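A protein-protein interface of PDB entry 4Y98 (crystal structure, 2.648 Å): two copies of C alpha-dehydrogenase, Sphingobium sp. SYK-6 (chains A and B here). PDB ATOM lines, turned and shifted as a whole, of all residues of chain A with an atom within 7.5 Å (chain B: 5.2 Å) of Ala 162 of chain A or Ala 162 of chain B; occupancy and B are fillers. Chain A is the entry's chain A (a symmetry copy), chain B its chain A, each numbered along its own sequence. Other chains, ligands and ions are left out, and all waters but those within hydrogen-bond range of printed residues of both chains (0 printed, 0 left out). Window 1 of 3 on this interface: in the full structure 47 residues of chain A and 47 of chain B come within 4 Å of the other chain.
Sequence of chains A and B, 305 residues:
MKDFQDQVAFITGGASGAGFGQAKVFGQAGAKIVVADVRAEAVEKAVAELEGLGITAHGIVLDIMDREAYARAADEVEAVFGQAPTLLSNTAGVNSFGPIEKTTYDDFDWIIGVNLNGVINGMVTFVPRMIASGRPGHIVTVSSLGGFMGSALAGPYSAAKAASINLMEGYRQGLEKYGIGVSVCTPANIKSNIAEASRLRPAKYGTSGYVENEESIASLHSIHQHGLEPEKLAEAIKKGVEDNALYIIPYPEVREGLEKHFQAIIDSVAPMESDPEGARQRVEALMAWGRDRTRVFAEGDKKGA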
ATOM      1  N   ASN A 115      -6.834 -31.887   2.167  1.00  0.00           N
ATOM      2  CA  ASN A 115      -6.962 -31.255   3.462  1.00  0.00           C
ATOM      3  C   ASN A 115      -8.401 -31.060   3.922  1.00  0.00           C
ATOM      4  O   ASN A 115      -8.642 -30.941   5.127  1.00  0.00           O
ATOM      5  CB  ASN A 115      -6.227 -29.920   3.443  1.00  0.00           C
ATOM      6  CG  ASN A 115      -4.718 -30.095   3.386  1.00  0.00           C
ATOM      7  OD1 ASN A 115      -4.098 -30.512   4.359  1.00  0.00           O
ATOM      8  ND2 ASN A 115      -4.123 -29.788   2.244  1.00  0.00           N
ATOM      9  N   LEU A 116      -9.350 -31.027   2.981  1.00  0.00           N
ATOM     10  CA  LEU A 116     -10.769 -31.009   3.338  1.00  0.00           C
ATOM     11  C   LEU A 116     -11.505 -32.253   2.866  1.00  0.00           C
ATOM     12  O   LEU A 116     -12.017 -33.012   3.680  1.00  0.00           O
ATOM     13  CB  LEU A 116     -11.465 -29.766   2.774  1.00  0.00           C
ATOM     14  CG  LEU A 116     -12.993 -29.695   2.965  1.00  0.00           C
ATOM     15  CD1 LEU A 116     -13.381 -29.940   4.418  1.00  0.00           C
ATOM     16  CD2 LEU A 116     -13.574 -28.355   2.491  1.00  0.00           C
ATOM     17  N   SER A 143      -5.606 -30.405  11.742  1.00  0.00           N
ATOM     18  CA  SER A 143      -5.813 -29.307  10.824  1.00  0.00           C
ATOM     19  C   SER A 143      -4.571 -28.422  10.844  1.00  0.00           C
ATOM     20  O   SER A 143      -3.472 -28.897  10.568  1.00  0.00           O
ATOM     21  CB  SER A 143      -7.077 -28.527  11.197  1.00  0.00           C
ATOM     22  OG  SER A 143      -7.338 -27.493  10.260  1.00  0.00           O
ATOM     23  N   SER A 144      -4.737 -27.144  11.170  1.00  0.00           N
ATOM     24  CA  SER A 144      -3.620 -26.204  11.174  1.00  0.00           C
ATOM     25  C   SER A 144      -4.006 -24.887  11.851  1.00  0.00           C
ATOM     26  O   SER A 144      -5.185 -24.546  11.951  1.00  0.00           O
ATOM     27  CB  SER A 144      -3.149 -25.935   9.744  1.00  0.00           C
ATOM     28  OG  SER A 144      -2.202 -24.882   9.689  1.00  0.00           O
ATOM     29  N   LEU A 145      -3.005 -24.161  12.330  1.00  0.00           N
ATOM     30  CA  LEU A 145      -3.214 -22.839  12.903  1.00  0.00           C
ATOM     31  C   LEU A 145      -3.626 -21.859  11.811  1.00  0.00           C
ATOM     32  O   LEU A 145      -4.311 -20.869  12.072  1.00  0.00           O
ATOM     33  CB  LEU A 145      -1.941 -22.364  13.591  1.00  0.00           C
ATOM     34  CG  LEU A 145      -2.060 -21.140  14.491  1.00  0.00           C
ATOM     35  CD1 LEU A 145      -2.693 -21.540  15.815  1.00  0.00           C
ATOM     36  CD2 LEU A 145      -0.688 -20.507  14.702  1.00  0.00           C
ATOM     37  N   GLY A 146      -3.183 -22.138  10.589  1.00  0.00           N
ATOM     38  CA  GLY A 146      -3.526 -21.324   9.437  1.00  0.00           C
ATOM     39  C   GLY A 146      -5.011 -21.388   9.173  1.00  0.00           C
ATOM     40  O   GLY A 146      -5.560 -20.552   8.463  1.00  0.00           O
ATOM     41  N   GLY A 147      -5.662 -22.394   9.749  1.00  0.00           N
ATOM     42  CA  GLY A 147      -7.104 -22.505   9.679  1.00  0.00           C
ATOM     43  C   GLY A 147      -7.795 -21.342  10.385  1.00  0.00           C
ATOM     44  O   GLY A 147      -8.918 -20.985  10.028  1.00  0.00           O
ATOM     45  N   PHE A 148      -7.126 -20.759  11.382  1.00  0.00           N
ATOM     46  CA  PHE A 148      -7.667 -19.624  12.137  1.00  0.00           C
ATOM     47  C   PHE A 148      -7.332 -18.274  11.494  1.00  0.00           C
ATOM     48  O   PHE A 148      -7.738 -17.227  11.996  1.00  0.00           O
ATOM     49  CB  PHE A 148      -7.135 -19.618  13.579  1.00  0.00           C
ATOM     50  CG  PHE A 148      -7.654 -20.734  14.443  1.00  0.00           C
ATOM     51  CD1 PHE A 148      -9.008 -20.999  14.541  1.00  0.00           C
ATOM     52  CD2 PHE A 148      -6.775 -21.509  15.185  1.00  0.00           C
ATOM     53  CE1 PHE A 148      -9.476 -22.029  15.352  1.00  0.00           C
ATOM     54  CE2 PHE A 148      -7.239 -22.531  15.995  1.00  0.00           C
ATOM     55  CZ  PHE A 148      -8.592 -22.789  16.077  1.00  0.00           C
ATOM     56  N   MET A 149      -6.576 -18.290  10.400  1.00  0.00           N
ATOM     57  CA  MET A 149      -6.142 -17.046   9.770  1.00  0.00           C
ATOM     58  C   MET A 149      -5.649 -17.252   8.336  1.00  0.00           C
ATOM     59  O   MET A 149      -4.578 -17.814   8.111  1.00  0.00           O
ATOM     60  CB  MET A 149      -5.042 -16.403  10.617  1.00  0.00           C
ATOM     61  CG  MET A 149      -4.063 -17.416  11.229  1.00  0.00           C
ATOM     62  SD  MET A 149      -2.710 -16.696  12.192  1.00  0.00           S
ATOM     63  CE  MET A 149      -3.609 -15.828  13.480  1.00  0.00           C
ATOM     64  N   GLY A 150      -6.440 -16.782   7.374  1.00  0.00           N
ATOM     65  CA  GLY A 150      -6.103 -16.894   5.960  1.00  0.00           C
ATOM     66  C   GLY A 150      -4.845 -16.135   5.560  1.00  0.00           C
ATOM     67  O   GLY A 150      -4.535 -15.085   6.128  1.00  0.00           O
ATOM     68  N   PRO A 156      -5.102 -21.566  -0.238  1.00  0.00           N
ATOM     69  CA  PRO A 156      -5.948 -22.757  -0.378  1.00  0.00           C
ATOM     70  C   PRO A 156      -5.850 -23.644   0.849  1.00  0.00           C
ATOM     71  O   PRO A 156      -6.881 -24.044   1.399  1.00  0.00           O
ATOM     72  CB  PRO A 156      -5.375 -23.467  -1.611  1.00  0.00           C
ATOM     73  CG  PRO A 156      -4.659 -22.413  -2.368  1.00  0.00           C
ATOM     74  CD  PRO A 156      -4.142 -21.436  -1.347  1.00  0.00           C
ATOM     75  N   TYR A 157      -4.618 -23.934   1.262  1.00  0.00           N
ATOM     76  CA  TYR A 157      -4.363 -24.782   2.407  1.00  0.00           C
ATOM     77  C   TYR A 157      -5.063 -24.239   3.646  1.00  0.00           C
ATOM     78  O   TYR A 157      -5.812 -24.962   4.303  1.00  0.00           O
ATOM     79  CB  TYR A 157      -2.850 -24.896   2.645  1.00  0.00           C
ATOM     80  CG  TYR A 157      -2.463 -25.707   3.867  1.00  0.00           C
ATOM     81  CD1 TYR A 157      -2.321 -27.081   3.791  1.00  0.00           C
ATOM     82  CD2 TYR A 157      -2.232 -25.093   5.091  1.00  0.00           C
ATOM     83  CE1 TYR A 157      -1.964 -27.825   4.897  1.00  0.00           C
ATOM     84  CE2 TYR A 157      -1.876 -25.832   6.213  1.00  0.00           C
ATOM     85  CZ  TYR A 157      -1.746 -27.198   6.105  1.00  0.00           C
ATOM     86  OH  TYR A 157      -1.395 -27.954   7.198  1.00  0.00           O
ATOM     87  N   SER A 158      -4.817 -22.968   3.955  1.00  0.00           N
ATOM     88  CA  SER A 158      -5.407 -22.336   5.139  1.00  0.00           C
ATOM     89  C   SER A 158      -6.925 -22.434   5.144  1.00  0.00           C
ATOM     90  O   SER A 158      -7.543 -22.632   6.189  1.00  0.00           O
ATOM     91  CB  SER A 158      -5.012 -20.861   5.231  1.00  0.00           C
ATOM     92  OG  SER A 158      -3.643 -20.707   5.564  1.00  0.00           O
ATOM     93  N   ALA A 159      -7.517 -22.288   3.969  1.00  0.00           N
ATOM     94  CA  ALA A 159      -8.960 -22.290   3.836  1.00  0.00           C
ATOM     95  C   ALA A 159      -9.544 -23.666   4.137  1.00  0.00           C
ATOM     96  O   ALA A 159     -10.558 -23.797   4.823  1.00  0.00           O
ATOM     97  CB  ALA A 159      -9.325 -21.857   2.464  1.00  0.00           C
ATOM     98  N   ALA A 160      -8.904 -24.696   3.606  1.00  0.00           N
ATOM     99  CA  ALA A 160      -9.341 -26.067   3.840  1.00  0.00           C
ATOM    100  C   ALA A 160      -9.228 -26.439   5.316  1.00  0.00           C
ATOM    101  O   ALA A 160     -10.092 -27.124   5.869  1.00  0.00           O
ATOM    102  CB  ALA A 160      -8.531 -27.010   3.002  1.00  0.00           C
ATOM    103  N   LYS A 161      -8.160 -25.976   5.950  1.00  0.00           N
ATOM    104  CA  LYS A 161      -7.943 -26.244   7.358  1.00  0.00           C
ATOM    105  C   LYS A 161      -8.963 -25.486   8.180  1.00  0.00           C
ATOM    106  O   LYS A 161      -9.431 -25.967   9.210  1.00  0.00           O
ATOM    107  CB  LYS A 161      -6.516 -25.857   7.746  1.00  0.00           C
ATOM    108  CG  LYS A 161      -5.485 -26.721   7.069  1.00  0.00           C
ATOM    109  CD  LYS A 161      -5.738 -28.201   7.315  1.00  0.00           C
ATOM    110  CE  LYS A 161      -4.509 -29.026   7.034  1.00  0.00           C
ATOM    111  NZ  LYS A 161      -4.847 -30.469   6.976  1.00  0.00           N
ATOM    112  N   ALA A 162      -9.328 -24.301   7.706  1.00  0.00           N
ATOM    113  CA  ALA A 162     -10.379 -23.517   8.352  1.00  0.00           C
ATOM    114  C   ALA A 162     -11.700 -24.274   8.359  1.00  0.00           C
ATOM    115  O   ALA A 162     -12.444 -24.236   9.337  1.00  0.00           O
ATOM    116  CB  ALA A 162     -10.548 -22.187   7.665  1.00  0.00           C
ATOM    117  N   ALA A 163     -11.990 -24.980   7.276  1.00  0.00           N
ATOM    118  CA  ALA A 163     -13.209 -25.782   7.219  1.00  0.00           C
ATOM    119  C   ALA A 163     -13.120 -27.038   8.103  1.00  0.00           C
ATOM    120  O   ALA A 163     -14.113 -27.438   8.711  1.00  0.00           O
ATOM    121  CB  ALA A 163     -13.511 -26.169   5.782  1.00  0.00           C
ATOM    122  N   SER A 164     -11.953 -27.666   8.192  1.00  0.00           N
ATOM    123  CA  SER A 164     -11.880 -28.901   8.966  1.00  0.00           C
ATOM    124  C   SER A 164     -12.053 -28.566  10.443  1.00  0.00           C
ATOM    125  O   SER A 164     -12.744 -29.284  11.175  1.00  0.00           O
ATOM    126  CB  SER A 164     -10.567 -29.651   8.718  1.00  0.00           C
ATOM    127  OG  SER A 164      -9.454 -28.967   9.252  1.00  0.00           O
ATOM    128  N   ILE A 165     -11.451 -27.463  10.877  1.00  0.00           N
ATOM    129  CA  ILE A 165     -11.656 -26.993  12.240  1.00  0.00           C
ATOM    130  C   ILE A 165     -13.145 -26.862  12.503  1.00  0.00           C
ATOM    131  O   ILE A 165     -13.680 -27.496  13.409  1.00  0.00           O
ATOM    132  CB  ILE A 165     -10.970 -25.640  12.501  1.00  0.00           C
ATOM    133  CG1 ILE A 165      -9.454 -25.797  12.417  1.00  0.00           C
ATOM    134  CG2 ILE A 165     -11.339 -25.110  13.888  1.00  0.00           C
ATOM    135  CD1 ILE A 165      -8.704 -24.485  12.373  1.00  0.00           C
ATOM    136  N   ASN A 166     -13.804 -26.050  11.684  1.00  0.00           N
ATOM    137  CA  ASN A 166     -15.240 -25.802  11.823  1.00  0.00           C
ATOM    138  C   ASN A 166     -16.058 -27.082  11.776  1.00  0.00           C
ATOM    139  O   ASN A 166     -16.953 -27.295  12.585  1.00  0.00           O
ATOM    140  CB  ASN A 166     -15.726 -24.855  10.724  1.00  0.00           C
ATOM    141  CG  ASN A 166     -17.175 -24.471  10.888  1.00  0.00           C
ATOM    142  OD1 ASN A 166     -18.094 -25.239  10.562  1.00  0.00           O
ATOM    143  ND2 ASN A 166     -17.394 -23.270  11.406  1.00  0.00           N
ATOM    144  N   LEU A 167     -15.743 -27.932  10.815  1.00  0.00           N
ATOM    145  CA  LEU A 167     -16.444 -29.190  10.664  1.00  0.00           C
ATOM    146  C   LEU A 167     -16.286 -30.068  11.909  1.00  0.00           C
ATOM    147  O   LEU A 167     -17.241 -30.724  12.334  1.00  0.00           O
ATOM    148  CB  LEU A 167     -15.929 -29.903   9.420  1.00  0.00           C
ATOM    149  CG  LEU A 167     -16.628 -31.192   9.009  1.00  0.00           C
ATOM    150  CD1 LEU A 167     -18.034 -30.892   8.570  1.00  0.00           C
ATOM    151  CD2 LEU A 167     -15.864 -31.867   7.882  1.00  0.00           C
ATOM    152  N   MET A 168     -15.090 -30.087  12.502  1.00  0.00           N
ATOM    153  CA  MET A 168     -14.915 -30.802  13.758  1.00  0.00           C
ATOM    154  C   MET A 168     -15.744 -30.136  14.853  1.00  0.00           C
ATOM    155  O   MET A 168     -16.314 -30.825  15.698  1.00  0.00           O
ATOM    156  CB  MET A 168     -13.446 -30.852  14.191  1.00  0.00           C
ATOM    157  CG  MET A 168     -12.537 -31.768  13.362  1.00  0.00           C
ATOM    158  SD  MET A 168     -13.172 -33.433  13.083  1.00  0.00           S
ATOM    159  CE  MET A 168     -13.760 -33.259  11.405  1.00  0.00           C
ATOM    160  N   GLU A 169     -15.800 -28.801  14.849  1.00  0.00           N
ATOM    161  CA  GLU A 169     -16.584 -28.082  15.852  1.00  0.00           C
ATOM    162  C   GLU A 169     -18.018 -28.585  15.782  1.00  0.00           C
ATOM    163  O   GLU A 169     -18.688 -28.732  16.805  1.00  0.00           O
ATOM    164  CB  GLU A 169     -16.550 -26.555  15.643  1.00  0.00           C
ATOM    165  CG  GLU A 169     -15.202 -25.867  15.914  1.00  0.00           C
ATOM    166  CD  GLU A 169     -15.187 -24.382  15.520  1.00  0.00           C
ATOM    167  OE1 GLU A 169     -15.974 -23.970  14.635  1.00  0.00           O
ATOM    168  OE2 GLU A 169     -14.383 -23.618  16.100  1.00  0.00           O
ATOM    169  N   SER B 143     -20.550 -14.711   3.169  1.00  0.00           N
ATOM    170  CA  SER B 143     -20.380 -15.989   3.823  1.00  0.00           C
ATOM    171  C   SER B 143     -21.465 -16.133   4.886  1.00  0.00           C
ATOM    172  O   SER B 143     -22.650 -16.064   4.569  1.00  0.00           O
ATOM    173  CB  SER B 143     -18.975 -16.105   4.422  1.00  0.00           C
ATOM    174  OG  SER B 143     -18.766 -17.384   4.999  1.00  0.00           O
ATOM    175  N   GLY B 147     -19.812 -19.518   9.839  1.00  0.00           N
ATOM    176  CA  GLY B 147     -18.440 -19.735   9.431  1.00  0.00           C
ATOM    177  C   GLY B 147     -17.475 -19.610  10.606  1.00  0.00           C
ATOM    178  O   GLY B 147     -16.406 -20.221  10.593  1.00  0.00           O
ATOM    179  N   TYR B 157     -22.690 -26.610   5.723  1.00  0.00           N
ATOM    180  CA  TYR B 157     -22.828 -25.209   5.386  1.00  0.00           C
ATOM    181  C   TYR B 157     -21.833 -24.365   6.172  1.00  0.00           C
ATOM    182  O   TYR B 157     -21.074 -23.594   5.586  1.00  0.00           O
ATOM    183  CB  TYR B 157     -24.266 -24.745   5.658  1.00  0.00           C
ATOM    184  CG  TYR B 157     -24.512 -23.270   5.406  1.00  0.00           C
ATOM    185  CD1 TYR B 157     -24.849 -22.812   4.145  1.00  0.00           C
ATOM    186  CD2 TYR B 157     -24.415 -22.342   6.434  1.00  0.00           C
ATOM    187  CE1 TYR B 157     -25.079 -21.471   3.909  1.00  0.00           C
ATOM    188  CE2 TYR B 157     -24.642 -20.989   6.209  1.00  0.00           C
ATOM    189  CZ  TYR B 157     -24.971 -20.565   4.941  1.00  0.00           C
ATOM    190  OH  TYR B 157     -25.200 -19.233   4.689  1.00  0.00           O
ATOM    191  N   SER B 158     -21.841 -24.518   7.494  1.00  0.00           N
ATOM    192  CA  SER B 158     -20.952 -23.744   8.365  1.00  0.00           C
ATOM    193  C   SER B 158     -19.490 -23.906   7.980  1.00  0.00           C
ATOM    194  O   SER B 158     -18.712 -22.954   8.034  1.00  0.00           O
ATOM    195  CB  SER B 158     -21.122 -24.152   9.829  1.00  0.00           C
ATOM    196  OG  SER B 158     -22.365 -23.721  10.351  1.00  0.00           O
ATOM    197  N   ALA B 159     -19.125 -25.119   7.597  1.00  0.00           N
ATOM    198  CA  ALA B 159     -17.750 -25.434   7.268  1.00  0.00           C
ATOM    199  C   ALA B 159     -17.307 -24.725   5.992  1.00  0.00           C
ATOM    200  O   ALA B 159     -16.205 -24.181   5.908  1.00  0.00           O
ATOM    201  CB  ALA B 159     -17.604 -26.904   7.124  1.00  0.00           C
ATOM    202  N   ALA B 160     -18.170 -24.746   4.988  1.00  0.00           N
ATOM    203  CA  ALA B 160     -17.883 -24.081   3.722  1.00  0.00           C
ATOM    204  C   ALA B 160     -17.754 -22.572   3.908  1.00  0.00           C
ATOM    205  O   ALA B 160     -16.899 -21.925   3.299  1.00  0.00           O
ATOM    206  CB  ALA B 160     -18.959 -24.393   2.728  1.00  0.00           C
ATOM    207  N   LYS B 161     -18.607 -22.018   4.759  1.00  0.00           N
ATOM    208  CA  LYS B 161     -18.578 -20.595   5.038  1.00  0.00           C
ATOM    209  C   LYS B 161     -17.325 -20.256   5.816  1.00  0.00           C
ATOM    210  O   LYS B 161     -16.734 -19.195   5.634  1.00  0.00           O
ATOM    211  CB  LYS B 161     -19.837 -20.191   5.804  1.00  0.00           C
ATOM    212  CG  LYS B 161     -21.087 -20.356   4.979  1.00  0.00           C
ATOM    213  CD  LYS B 161     -20.991 -19.615   3.654  1.00  0.00           C
ATOM    214  CE  LYS B 161     -22.350 -19.403   3.039  1.00  0.00           C
ATOM    215  NZ  LYS B 161     -22.226 -18.966   1.627  1.00  0.00           N
ATOM    216  N   ALA B 162     -16.905 -21.181   6.671  1.00  0.00           N
ATOM    217  CA  ALA B 162     -15.653 -21.018   7.407  1.00  0.00           C
ATOM    218  C   ALA B 162     -14.469 -20.907   6.456  1.00  0.00           C
ATOM    219  O   ALA B 162     -13.550 -20.122   6.681  1.00  0.00           O
ATOM    220  CB  ALA B 162     -15.444 -22.165   8.363  1.00  0.00           C
ATOM    221  N   ALA B 163     -14.493 -21.680   5.379  1.00  0.00           N
ATOM    222  CA  ALA B 163     -13.428 -21.599   4.386  1.00  0.00           C
ATOM    223  C   ALA B 163     -13.509 -20.308   3.551  1.00  0.00           C
ATOM    224  O   ALA B 163     -12.479 -19.734   3.198  1.00  0.00           O
ATOM    225  CB  ALA B 163     -13.466 -22.815   3.480  1.00  0.00           C
ATOM    226  N   SER B 164     -14.709 -19.838   3.231  1.00  0.00           N
ATOM    227  CA  SER B 164     -14.794 -18.659   2.376  1.00  0.00           C
ATOM    228  C   SER B 164     -14.292 -17.448   3.156  1.00  0.00           C
ATOM    229  O   SER B 164     -13.575 -16.602   2.611  1.00  0.00           O
ATOM    230  CB  SER B 164     -16.218 -18.433   1.858  1.00  0.00           C
ATOM    231  OG  SER B 164     -17.105 -18.047   2.888  1.00  0.00           O
ATOM    232  N   ILE B 165     -14.645 -17.378   4.436  1.00  0.00           N
ATOM    233  CA  ILE B 165     -14.117 -16.327   5.294  1.00  0.00           C
ATOM    234  C   ILE B 165     -12.602 -16.333   5.214  1.00  0.00           C
ATOM    235  O   ILE B 165     -11.989 -15.336   4.836  1.00  0.00           O
ATOM    236  CB  ILE B 165     -14.552 -16.497   6.760  1.00  0.00           C
ATOM    237  CG1 ILE B 165     -16.062 -16.313   6.884  1.00  0.00           C
ATOM    238  CG2 ILE B 165     -13.852 -15.468   7.651  1.00  0.00           C
ATOM    239  CD1 ILE B 165     -16.624 -16.739   8.221  1.00  0.00           C
ATOM    240  N   ASN B 166     -12.013 -17.475   5.550  1.00  0.00           N
ATOM    241  CA  ASN B 166     -10.558 -17.630   5.545  1.00  0.00           C
ATOM    242  C   ASN B 166      -9.943 -17.309   4.194  1.00  0.00           C
ATOM    243  O   ASN B 166      -8.944 -16.606   4.100  1.00  0.00           O
ATOM    244  CB  ASN B 166     -10.174 -19.057   5.945  1.00  0.00           C
ATOM    245  CG  ASN B 166      -8.682 -19.242   6.072  1.00  0.00           C
ATOM    246  OD1 ASN B 166      -7.956 -19.380   5.076  1.00  0.00           O
ATOM    247  ND2 ASN B 166      -8.207 -19.240   7.311  1.00  0.00           N
ATOM    248  N   LEU B 167     -10.551 -17.835   3.145  1.00  0.00           N
ATOM    249  CA  LEU B 167     -10.067 -17.602   1.801  1.00  0.00           C
ATOM    250  C   LEU B 167     -10.095 -16.110   1.450  1.00  0.00           C
ATOM    251  O   LEU B 167      -9.172 -15.605   0.807  1.00  0.00           O
ATOM    252  CB  LEU B 167     -10.905 -18.411   0.820  1.00  0.00           C
ATOM    253  CG  LEU B 167     -10.479 -18.406  -0.642  1.00  0.00           C
ATOM    254  CD1 LEU B 167      -9.159 -19.108  -0.791  1.00  0.00           C
ATOM    255  CD2 LEU B 167     -11.532 -19.089  -1.499  1.00  0.00           C
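Among the printed residues, merely in contact across the chains: Met 149 of chain A with Asn 166 of chain B, Ala 159 of chain A with Ala 163 of chain B, Ala 162 of chain A with Ala 162 of chain B, Ala 162 of chain A with Asn 166 of chain B, Ala 163 of chain A with Ala 159 of chain B and Asn 166 of chain A with Ala 162 of chain B.
Of the 24 printed residues of chain A, 9 touch a printed residue of chain B.
Printed residues of chain A that touch a printed residue of chain B: Gly 146, Gly 147, Met 149, Gly 150, Ser 158, Ala 159, Ala 162, Ala 163 and Asn 166.
Of the 13 printed residues of chain B, 6 touch a printed residue of chain A.
Among the printed residues, 14 pairs touch across the chains.
ND2 of Asn 166 of chain B sits close to N of Gly 150 of chain A, 3.0 Å away.
The side-chain amide oxygen of Asn 166 of chain B sits at hydrogen-bond distance from the backbone NH of Ala 159 of chain A.
The side-chain amide oxygen (OD1) of Asn 166 of chain A lies close to the backbone carbonyl oxygen (O) of Ser 158 of chain B (3.5 Å).
The side-chain amide oxygen (OD1) of Asn 166 of chain B lies close to the backbone carbonyl oxygen (O) of Ser 158 of chain A, 3.5 Å away.
ND2 of Asn 166 of chain B is in hydrogen-bond range of O of Gly 147 of chain A (3.3 Å).
O of Gly 147 of chain B is in hydrogen-bond range of ND2 of Asn 166 of chain A.
The backbone NH (N) of Ala 159 of chain B sits at hydrogen-bond distance from the side-chain amide oxygen (OD1) of Asn 166 of chain A.
The side-chain amide nitrogen (ND2) of Asn 166 of chain B is in hydrogen-bond range of the backbone carbonyl oxygen (O) of Gly 146 of chain A (3.2 Å).
Printed residues of chain B within 4 Å of Met 149 of chain A: Asn 166.
Tyr 157 of chain A touches none of the printed residues of chain B.
Ala 162 of chain A touches just these residues of chain B: Ala 162 and Asn 166.
Ala 162 of chain B touches just these residues of chain A: Ala 162 and Asn 166.
Printed residues of chain A within 4 Å of Ala 163 of chain B: Ala 159.
Ile 165 of chain B touches none of the printed residues of chain A.
The nearest residue of chain A that does not touch Ala 162 of chain B is Ala 163 of chain A (4.4 Å).
The backbone carbonyl oxygen (O) of Gly 146 of chain A sits close to the side-chain hydroxyl (OG) of Ser 158 of chain A, at 3.5 Å.
N of Gly 146 of chain A is in hydrogen-bond range of OG of Ser 144 of chain A, 3.0 Å away.
Gly 147 of chain A touches Asn 166 of chain B, and with the chains exchanged Asn 166 of chain A touches Gly 147 of chain B.
Ser 158 of chain A touches Asn 166 of chain B, and with the chains exchanged Asn 166 of chain A touches Ser 158 of chain B.
Ala 159 of chain A touches Asn 166 of chain B, and with the chains exchanged Asn 166 of chain A touches Ala 159 of chain B.
Ala 162 of chain A touches its own counterpart, Ala 162 of chain B.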
